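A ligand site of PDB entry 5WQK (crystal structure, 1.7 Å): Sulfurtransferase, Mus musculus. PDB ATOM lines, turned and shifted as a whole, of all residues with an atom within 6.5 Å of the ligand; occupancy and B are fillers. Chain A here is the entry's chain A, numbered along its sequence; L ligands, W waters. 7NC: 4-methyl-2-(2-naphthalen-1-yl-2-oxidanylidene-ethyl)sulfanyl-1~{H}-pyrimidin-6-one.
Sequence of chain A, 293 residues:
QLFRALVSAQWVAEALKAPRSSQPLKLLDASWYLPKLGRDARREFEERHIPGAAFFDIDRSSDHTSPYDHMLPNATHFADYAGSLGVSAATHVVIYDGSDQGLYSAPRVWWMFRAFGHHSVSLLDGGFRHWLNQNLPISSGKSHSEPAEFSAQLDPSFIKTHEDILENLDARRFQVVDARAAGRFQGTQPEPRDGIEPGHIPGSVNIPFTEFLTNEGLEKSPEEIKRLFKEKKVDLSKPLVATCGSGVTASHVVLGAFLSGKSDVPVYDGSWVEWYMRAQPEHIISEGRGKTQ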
ATOM      1  N   TRP A  32     -11.280 -29.636   2.751  1.00  0.00           N
ATOM      2  CA  TRP A  32     -12.669 -29.141   2.406  1.00  0.00           C
ATOM      3  C   TRP A  32     -12.808 -27.783   3.039  1.00  0.00           C
ATOM      4  O   TRP A  32     -12.327 -27.612   4.143  1.00  0.00           O
ATOM      5  CB  TRP A  32     -13.752 -30.129   2.945  1.00  0.00           C
ATOM      6  CG  TRP A  32     -15.136 -29.807   2.440  1.00  0.00           C
ATOM      7  CD1 TRP A  32     -15.754 -30.351   1.368  1.00  0.00           C
ATOM      8  CD2 TRP A  32     -16.067 -28.848   2.977  1.00  0.00           C
ATOM      9  NE1 TRP A  32     -16.978 -29.782   1.157  1.00  0.00           N
ATOM     10  CE2 TRP A  32     -17.187 -28.834   2.119  1.00  0.00           C
ATOM     11  CE3 TRP A  32     -16.005 -27.957   4.040  1.00  0.00           C
ATOM     12  CZ2 TRP A  32     -18.298 -28.018   2.373  1.00  0.00           C
ATOM     13  CZ3 TRP A  32     -17.150 -27.133   4.280  1.00  0.00           C
ATOM     14  CH2 TRP A  32     -18.239 -27.211   3.452  1.00  0.00           C
ATOM     15  N   LEU A  34     -15.285 -24.064   3.535  1.00  0.00           N
ATOM     16  CA  LEU A  34     -16.604 -23.447   3.370  1.00  0.00           C
ATOM     17  C   LEU A  34     -16.491 -22.503   2.146  1.00  0.00           C
ATOM     18  O   LEU A  34     -15.393 -21.953   1.865  1.00  0.00           O
ATOM     19  CB  LEU A  34     -16.871 -22.662   4.640  1.00  0.00           C
ATOM     20  CG  LEU A  34     -17.319 -23.515   5.858  1.00  0.00           C
ATOM     21  CD1 LEU A  34     -17.259 -22.694   7.096  1.00  0.00           C
ATOM     22  CD2 LEU A  34     -18.659 -24.117   5.618  1.00  0.00           C
ATOM     23  N   PRO A  35     -17.602 -22.339   1.417  1.00  0.00           N
ATOM     24  CA  PRO A  35     -17.554 -21.585   0.144  1.00  0.00           C
ATOM     25  C   PRO A  35     -16.969 -20.205   0.273  1.00  0.00           C
ATOM     26  O   PRO A  35     -16.239 -19.775  -0.601  1.00  0.00           O
ATOM     27  CB  PRO A  35     -19.038 -21.520  -0.297  1.00  0.00           C
ATOM     28  CG  PRO A  35     -19.738 -22.670   0.444  1.00  0.00           C
ATOM     29  CD  PRO A  35     -18.904 -23.051   1.632  1.00  0.00           C
ATOM     30  N   ILE A  58     -14.719 -35.351   0.924  1.00  0.00           N
ATOM     31  CA  ILE A  58     -15.758 -35.626   1.950  1.00  0.00           C
ATOM     32  C   ILE A  58     -17.167 -35.452   1.395  1.00  0.00           C
ATOM     33  O   ILE A  58     -18.074 -36.055   1.886  1.00  0.00           O
ATOM     34  CB  ILE A  58     -15.555 -34.872   3.259  1.00  0.00           C
ATOM     35  CG1 ILE A  58     -15.702 -33.383   3.109  1.00  0.00           C
ATOM     36  CG2 ILE A  58     -14.178 -35.165   3.798  1.00  0.00           C
ATOM     37  CD1 ILE A  58     -15.934 -32.694   4.401  1.00  0.00           C
ATOM     38  N   ASP A  59     -17.348 -34.707   0.298  1.00  0.00           N
ATOM     39  CA  ASP A  59     -18.623 -34.795  -0.488  1.00  0.00           C
ATOM     40  C   ASP A  59     -18.940 -36.087  -1.275  1.00  0.00           C
ATOM     41  O   ASP A  59     -20.067 -36.249  -1.695  1.00  0.00           O
ATOM     42  CB  ASP A  59     -18.744 -33.592  -1.396  1.00  0.00           C
ATOM     43  CG  ASP A  59     -18.823 -32.298  -0.624  1.00  0.00           C
ATOM     44  OD1 ASP A  59     -19.468 -32.258   0.451  1.00  0.00           O
ATOM     45  OD2 ASP A  59     -18.277 -31.316  -1.131  1.00  0.00           O
ATOM     46  N   ASP A  69     -26.256 -31.434   6.466  1.00  0.00           N
ATOM     47  CA  ASP A  69     -24.950 -31.383   5.864  1.00  0.00           C
ATOM     48  C   ASP A  69     -23.964 -32.405   6.419  1.00  0.00           C
ATOM     49  O   ASP A  69     -24.035 -32.868   7.596  1.00  0.00           O
ATOM     50  CB  ASP A  69     -24.417 -29.977   6.000  1.00  0.00           C
ATOM     51  CG  ASP A  69     -25.180 -28.972   5.135  1.00  0.00           C
ATOM     52  OD1 ASP A  69     -25.378 -29.274   3.980  1.00  0.00           O
ATOM     53  OD2 ASP A  69     -25.342 -27.845   5.623  1.00  0.00           O
ATOM     54  N   HIS A  70     -23.100 -32.882   5.512  1.00  0.00           N
ATOM     55  CA  HIS A  70     -22.013 -33.788   5.891  1.00  0.00           C
ATOM     56  C   HIS A  70     -22.419 -34.956   6.773  1.00  0.00           C
ATOM     57  O   HIS A  70     -21.806 -35.181   7.832  1.00  0.00           O
ATOM     58  CB  HIS A  70     -20.840 -33.035   6.517  1.00  0.00           C
ATOM     59  CG  HIS A  70     -20.204 -32.033   5.611  1.00  0.00           C
ATOM     60  ND1 HIS A  70     -19.786 -32.386   4.347  1.00  0.00           N
ATOM     61  CD2 HIS A  70     -19.917 -30.735   5.759  1.00  0.00           C
ATOM     62  CE1 HIS A  70     -19.302 -31.340   3.725  1.00  0.00           C
ATOM     63  NE2 HIS A  70     -19.348 -30.319   4.556  1.00  0.00           N
ATOM     64  N   TYR A 104      -8.231 -29.267   9.856  1.00  0.00           N
ATOM     65  CA  TYR A 104      -9.521 -28.697   9.853  1.00  0.00           C
ATOM     66  C   TYR A 104     -10.612 -29.726   9.609  1.00  0.00           C
ATOM     67  O   TYR A 104     -11.432 -30.027  10.463  1.00  0.00           O
ATOM     68  CB  TYR A 104      -9.577 -27.570   8.814  1.00  0.00           C
ATOM     69  CG  TYR A 104     -10.970 -26.949   8.623  1.00  0.00           C
ATOM     70  CD1 TYR A 104     -11.460 -26.016   9.527  1.00  0.00           C
ATOM     71  CD2 TYR A 104     -11.721 -27.242   7.496  1.00  0.00           C
ATOM     72  CE1 TYR A 104     -12.731 -25.406   9.371  1.00  0.00           C
ATOM     73  CE2 TYR A 104     -12.979 -26.670   7.325  1.00  0.00           C
ATOM     74  CZ  TYR A 104     -13.486 -25.759   8.263  1.00  0.00           C
ATOM     75  OH  TYR A 104     -14.701 -25.133   8.026  1.00  0.00           O
ATOM     76  N   ARG A 180     -17.930 -24.904  17.211  1.00  0.00           N
ATOM     77  CA  ARG A 180     -18.000 -23.724  16.370  1.00  0.00           C
ATOM     78  C   ARG A 180     -17.274 -22.524  17.037  1.00  0.00           C
ATOM     79  O   ARG A 180     -17.073 -22.488  18.253  1.00  0.00           O
ATOM     80  CB  ARG A 180     -19.460 -23.379  16.120  1.00  0.00           C
ATOM     81  CG  ARG A 180     -20.056 -24.308  15.140  1.00  0.00           C
ATOM     82  CD  ARG A 180     -21.572 -24.059  14.976  1.00  0.00           C
ATOM     83  NE  ARG A 180     -22.244 -24.164  16.249  1.00  0.00           N
ATOM     84  CZ  ARG A 180     -23.229 -23.377  16.723  1.00  0.00           C
ATOM     85  NH1 ARG A 180     -23.722 -22.412  15.991  1.00  0.00           N
ATOM     86  NH2 ARG A 180     -23.734 -23.582  17.906  1.00  0.00           N
ATOM     87  N   ALA A 181     -16.894 -21.553  16.209  1.00  0.00           N
ATOM     88  CA  ALA A 181     -16.450 -20.247  16.724  1.00  0.00           C
ATOM     89  C   ALA A 181     -17.408 -19.667  17.694  1.00  0.00           C
ATOM     90  O   ALA A 181     -18.636 -19.816  17.566  1.00  0.00           O
ATOM     91  CB  ALA A 181     -16.288 -19.278  15.549  1.00  0.00           C
ATOM     92  N   ARG A 184     -20.578 -17.625  16.524  1.00  0.00           N
ATOM     93  CA  ARG A 184     -21.676 -18.502  16.068  1.00  0.00           C
ATOM     94  C   ARG A 184     -22.389 -19.205  17.229  1.00  0.00           C
ATOM     95  O   ARG A 184     -23.668 -19.224  17.372  1.00  0.00           O
ATOM     96  CB  ARG A 184     -21.142 -19.484  15.048  1.00  0.00           C
ATOM     97  CG  ARG A 184     -20.789 -18.889  13.710  1.00  0.00           C
ATOM     98  CD  ARG A 184     -20.016 -19.871  12.849  1.00  0.00           C
ATOM     99  NE  ARG A 184     -20.798 -21.055  12.478  1.00  0.00           N
ATOM    100  CZ  ARG A 184     -20.285 -22.135  11.920  1.00  0.00           C
ATOM    101  NH1 ARG A 184     -19.009 -22.156  11.526  1.00  0.00           N
ATOM    102  NH2 ARG A 184     -21.099 -23.167  11.636  1.00  0.00           N
ATOM    103  N   GLU A 191     -24.150 -18.004  10.542  1.00  0.00           N
ATOM    104  CA  GLU A 191     -23.918 -19.352  10.106  1.00  0.00           C
ATOM    105  C   GLU A 191     -23.693 -19.370   8.578  1.00  0.00           C
ATOM    106  O   GLU A 191     -24.406 -18.699   7.844  1.00  0.00           O
ATOM    107  CB  GLU A 191     -25.117 -20.252  10.447  1.00  0.00           C
ATOM    108  CG  GLU A 191     -25.232 -20.611  11.909  1.00  0.00           C
ATOM    109  CD  GLU A 191     -24.118 -21.592  12.308  1.00  0.00           C
ATOM    110  OE1 GLU A 191     -23.886 -22.604  11.587  1.00  0.00           O
ATOM    111  OE2 GLU A 191     -23.556 -21.313  13.339  1.00  0.00           O
ATOM    112  N   PRO A 192     -22.790 -20.235   8.102  1.00  0.00           N
ATOM    113  CA  PRO A 192     -22.482 -20.298   6.672  1.00  0.00           C
ATOM    114  C   PRO A 192     -23.620 -20.748   5.770  1.00  0.00           C
ATOM    115  O   PRO A 192     -23.722 -20.272   4.610  1.00  0.00           O
ATOM    116  CB  PRO A 192     -21.266 -21.229   6.568  1.00  0.00           C
ATOM    117  CG  PRO A 192     -21.209 -21.904   7.921  1.00  0.00           C
ATOM    118  CD  PRO A 192     -21.836 -20.997   8.906  1.00  0.00           C
ATOM    119  N   ARG A 193     -24.504 -21.621   6.286  1.00  0.00           N
ATOM    120  CA  ARG A 193     -25.628 -22.113   5.498  1.00  0.00           C
ATOM    121  C   ARG A 193     -26.759 -21.055   5.474  1.00  0.00           C
ATOM    122  O   ARG A 193     -27.164 -20.519   6.530  1.00  0.00           O
ATOM    123  CB  ARG A 193     -26.061 -23.453   6.084  1.00  0.00           C
ATOM    124  CG  ARG A 193     -27.138 -24.224   5.379  1.00  0.00           C
ATOM    125  CD  ARG A 193     -26.683 -24.498   3.985  1.00  0.00           C
ATOM    126  NE  ARG A 193     -26.004 -25.757   3.740  1.00  0.00           N
ATOM    127  CZ  ARG A 193     -25.790 -26.160   2.496  1.00  0.00           C
ATOM    128  NH1 ARG A 193     -26.193 -25.335   1.498  1.00  0.00           N
ATOM    129  NH2 ARG A 193     -25.271 -27.326   2.211  1.00  0.00           N
ATOM    130  N   ASP A 194     -27.233 -20.714   4.265  1.00  0.00           N
ATOM    131  CA  ASP A 194     -28.342 -19.803   4.171  1.00  0.00           C
ATOM    132  C   ASP A 194     -29.574 -20.474   4.746  1.00  0.00           C
ATOM    133  O   ASP A 194     -29.808 -21.644   4.486  1.00  0.00           O
ATOM    134  CB  ASP A 194     -28.655 -19.384   2.752  1.00  0.00           C
ATOM    135  CG  ASP A 194     -29.857 -18.450   2.701  1.00  0.00           C
ATOM    136  OD1 ASP A 194     -30.783 -18.770   1.932  1.00  0.00           O
ATOM    137  OD2 ASP A 194     -29.885 -17.425   3.441  1.00  0.00           O
ATOM    138  N   PHE A 209     -12.905 -25.245  17.887  1.00  0.00           N
ATOM    139  CA  PHE A 209     -11.911 -26.261  17.502  1.00  0.00           C
ATOM    140  C   PHE A 209     -10.508 -25.723  17.480  1.00  0.00           C
ATOM    141  O   PHE A 209      -9.569 -26.451  17.759  1.00  0.00           O
ATOM    142  CB  PHE A 209     -12.226 -26.914  16.170  1.00  0.00           C
ATOM    143  CG  PHE A 209     -12.015 -26.033  14.959  1.00  0.00           C
ATOM    144  CD1 PHE A 209     -13.050 -25.211  14.507  1.00  0.00           C
ATOM    145  CD2 PHE A 209     -10.822 -25.991  14.324  1.00  0.00           C
ATOM    146  CE1 PHE A 209     -12.872 -24.429  13.386  1.00  0.00           C
ATOM    147  CE2 PHE A 209     -10.646 -25.239  13.212  1.00  0.00           C
ATOM    148  CZ  PHE A 209     -11.679 -24.426  12.764  1.00  0.00           C
ATOM    149  N   CSS A 244     -20.918 -29.331  16.149  1.00  0.00           N
ATOM    150  CA  CSS A 244     -20.411 -28.164  15.461  1.00  0.00           C
ATOM    151  CB  CSS A 244     -19.028 -28.472  14.865  1.00  0.00           C
ATOM    152  SG  CSS A 244     -19.008 -29.604  13.504  1.00  0.00           S
ATOM    153  SD  CSS A 244     -18.619 -28.436  11.768  1.00  0.00           S
ATOM    154  C   CSS A 244     -21.467 -27.722  14.466  1.00  0.00           C
ATOM    155  O   CSS A 244     -22.655 -27.818  14.798  1.00  0.00           O
ATOM    156  N   GLY A 245     -21.072 -27.213  13.276  1.00  0.00           N
ATOM    157  CA  GLY A 245     -22.015 -26.763  12.291  1.00  0.00           C
ATOM    158  C   GLY A 245     -22.668 -27.998  11.610  1.00  0.00           C
ATOM    159  O   GLY A 245     -23.893 -28.084  11.512  1.00  0.00           O
ATOM    160  N   SER A 246     -21.816 -28.917  11.120  1.00  0.00           N
ATOM    161  CA  SER A 246     -22.273 -30.048  10.306  1.00  0.00           C
ATOM    162  C   SER A 246     -21.670 -31.369  10.726  1.00  0.00           C
ATOM    163  O   SER A 246     -21.847 -32.381   9.993  1.00  0.00           O
ATOM    164  CB  SER A 246     -22.078 -29.767   8.813  1.00  0.00           C
ATOM    165  OG  SER A 246     -20.647 -29.688   8.473  1.00  0.00           O
ATOM    166  N   GLY A 247     -20.916 -31.378  11.826  1.00  0.00           N
ATOM    167  CA  GLY A 247     -20.276 -32.626  12.369  1.00  0.00           C
ATOM    168  C   GLY A 247     -18.824 -32.860  11.906  1.00  0.00           C
ATOM    169  O   GLY A 247     -18.298 -33.956  12.129  1.00  0.00           O
ATOM    170  N   VAL A 248     -18.234 -31.850  11.256  1.00  0.00           N
ATOM    171  CA  VAL A 248     -16.872 -31.998  10.689  1.00  0.00           C
ATOM    172  C   VAL A 248     -15.878 -31.526  11.762  1.00  0.00           C
ATOM    173  O   VAL A 248     -15.115 -32.346  12.320  1.00  0.00           O
ATOM    174  CB  VAL A 248     -16.734 -31.177   9.439  1.00  0.00           C
ATOM    175  CG1 VAL A 248     -15.316 -31.097   8.952  1.00  0.00           C
ATOM    176  CG2 VAL A 248     -17.631 -31.745   8.314  1.00  0.00           C
ATOM    177  N   THR A 249     -15.923 -30.264  12.103  1.00  0.00           N
ATOM    178  CA  THR A 249     -14.960 -29.718  13.091  1.00  0.00           C
ATOM    179  C   THR A 249     -15.148 -30.255  14.532  1.00  0.00           C
ATOM    180  O   THR A 249     -14.207 -30.209  15.322  1.00  0.00           O
ATOM    181  CB  THR A 249     -14.893 -28.169  13.114  1.00  0.00           C
ATOM    182  OG1 THR A 249     -16.124 -27.608  13.619  1.00  0.00           O
ATOM    183  CG2 THR A 249     -14.540 -27.591  11.744  1.00  0.00           C
ATOM    184  N   VAL A 273     -26.837 -27.472  12.006  1.00  0.00           N
ATOM    185  CA  VAL A 273     -27.723 -27.392  10.880  1.00  0.00           C
ATOM    186  C   VAL A 273     -29.000 -28.177  11.189  1.00  0.00           C
ATOM    187  O   VAL A 273     -30.105 -27.720  10.973  1.00  0.00           O
ATOM    188  CB  VAL A 273     -27.035 -27.816   9.558  1.00  0.00           C
ATOM    189  CG1 VAL A 273     -28.021 -28.051   8.404  1.00  0.00           C
ATOM    190  CG2 VAL A 273     -26.040 -26.717   9.160  1.00  0.00           C
HETATM  191  O1  7NC L   1     -22.141 -24.515   6.408  1.00  0.00           O
HETATM  192  C2  7NC L   1     -22.287 -25.727   6.160  1.00  0.00           C
HETATM  193  C3  7NC L   1     -22.517 -26.696   7.301  1.00  0.00           C
HETATM  194  S   7NC L   1     -22.213 -25.888   8.821  1.00  0.00           S
HETATM  195  C4  7NC L   1     -20.502 -26.012   8.983  1.00  0.00           C
HETATM  196  N1  7NC L   1     -19.813 -25.258   9.850  1.00  0.00           N
HETATM  197  C7  7NC L   1     -18.510 -25.326   9.994  1.00  0.00           C
HETATM  198  O   7NC L   1     -17.903 -24.537  10.768  1.00  0.00           O
HETATM  199  C6  7NC L   1     -17.818 -26.241   9.231  1.00  0.00           C
HETATM  200  N   7NC L   1     -19.854 -26.936   8.244  1.00  0.00           N
HETATM  201  C5  7NC L   1     -18.523 -27.025   8.377  1.00  0.00           C
HETATM  202  C8  7NC L   1     -17.781 -28.074   7.621  1.00  0.00           C
HETATM  203  C1  7NC L   1     -22.162 -26.219   4.763  1.00  0.00           C
HETATM  204  C11 7NC L   1     -21.851 -27.551   4.499  1.00  0.00           C
HETATM  205  C12 7NC L   1     -21.802 -28.072   3.212  1.00  0.00           C
HETATM  206  C10 7NC L   1     -21.993 -27.268   2.100  1.00  0.00           C
HETATM  207  C9  7NC L   1     -22.327 -25.930   2.232  1.00  0.00           C
HETATM  208  C16 7NC L   1     -22.550 -25.158   1.097  1.00  0.00           C
HETATM  209  C15 7NC L   1     -22.902 -23.823   1.319  1.00  0.00           C
HETATM  210  C14 7NC L   1     -22.956 -23.222   2.561  1.00  0.00           C
HETATM  211  C13 7NC L   1     -22.787 -23.959   3.723  1.00  0.00           C
HETATM  212  C   7NC L   1     -22.422 -25.312   3.592  1.00  0.00           C
HETATM  213  O   HOH W   1     -24.404 -23.239   8.816  1.00  0.00           O
HETATM  214  O   HOH W   2     -16.822 -24.964  13.283  1.00  0.00           O
HETATM  215  O   HOH W   3     -15.617 -23.813  10.152  1.00  0.00           O
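Trp 32 touches the ligand. Leu 34 touches the ligand (CD2 to O1, 3.6 Å). CG of Pro 35 touches C15 of the ligand (3.5 Å). OD2 of Asp 69 touches C3 of the ligand, at 3.5 Å. His 70 touches the ligand. Tyr 104 touches the ligand. CG of Pro 192 touches O1 of the ligand (3.2 Å). NH2 of Arg 193 touches C9 of the ligand, 3.3 Å away. CSS 244 touches the ligand (SD to C6, 3.4 Å). Gly 245 touches the ligand. Val 248 touches the ligand (CG2 to C8, 3.7 Å). Val 273 touches the ligand.
Water W3 lies within hydrogen-bond range of O of the ligand (2.5 Å) and OH of Tyr 104 (2.7 Å). Water W2 bridges OG1 of Thr 249 and O of the ligand. Water W1 lies within hydrogen-bond range of OE1 of Glu 191 (2.9 Å), N of Arg 193 (3.0 Å) and S of the ligand (3.4 Å).
O of the ligand is in hydrogen-bond range of NH1 of Arg 184 (2.7 Å). A nitrogen (N) of the ligand is in hydrogen-bond range of the side-chain hydroxyl (OG) of Ser 246 (2.9 Å).
SD of CSS 244 is in hydrogen-bond range of N of Ser 246 (3.3 Å). The side-chain carboxylate (OE1) of Glu 191 lies within salt-bridge range of the guanidinium group (NH2) of Arg 184, 2.8 Å away. The guanidinium group (NH2) of Arg 193 is in salt-bridge range of the side-chain carboxylate (OD1) of Asp 69, at 2.6 Å. NE1 of Trp 32 lies within hydrogen-bond range of OD2 of Asp 59 (3.0 Å). SG of CSS 244 sits at hydrogen-bond distance from the backbone NH (N) of Gly 247, at 3.1 Å. The backbone carbonyl oxygen of Gly 245 sits at hydrogen-bond distance from the backbone NH of Val 273. SD of CSS 244 lies within hydrogen-bond range of the side-chain hydroxyl (OG1) of Thr 249 (3.2 Å). The backbone carbonyl oxygen (O) of Arg 184 lies within hydrogen-bond range of the guanidinium group (NH1) of Arg 180 (3.5 Å).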
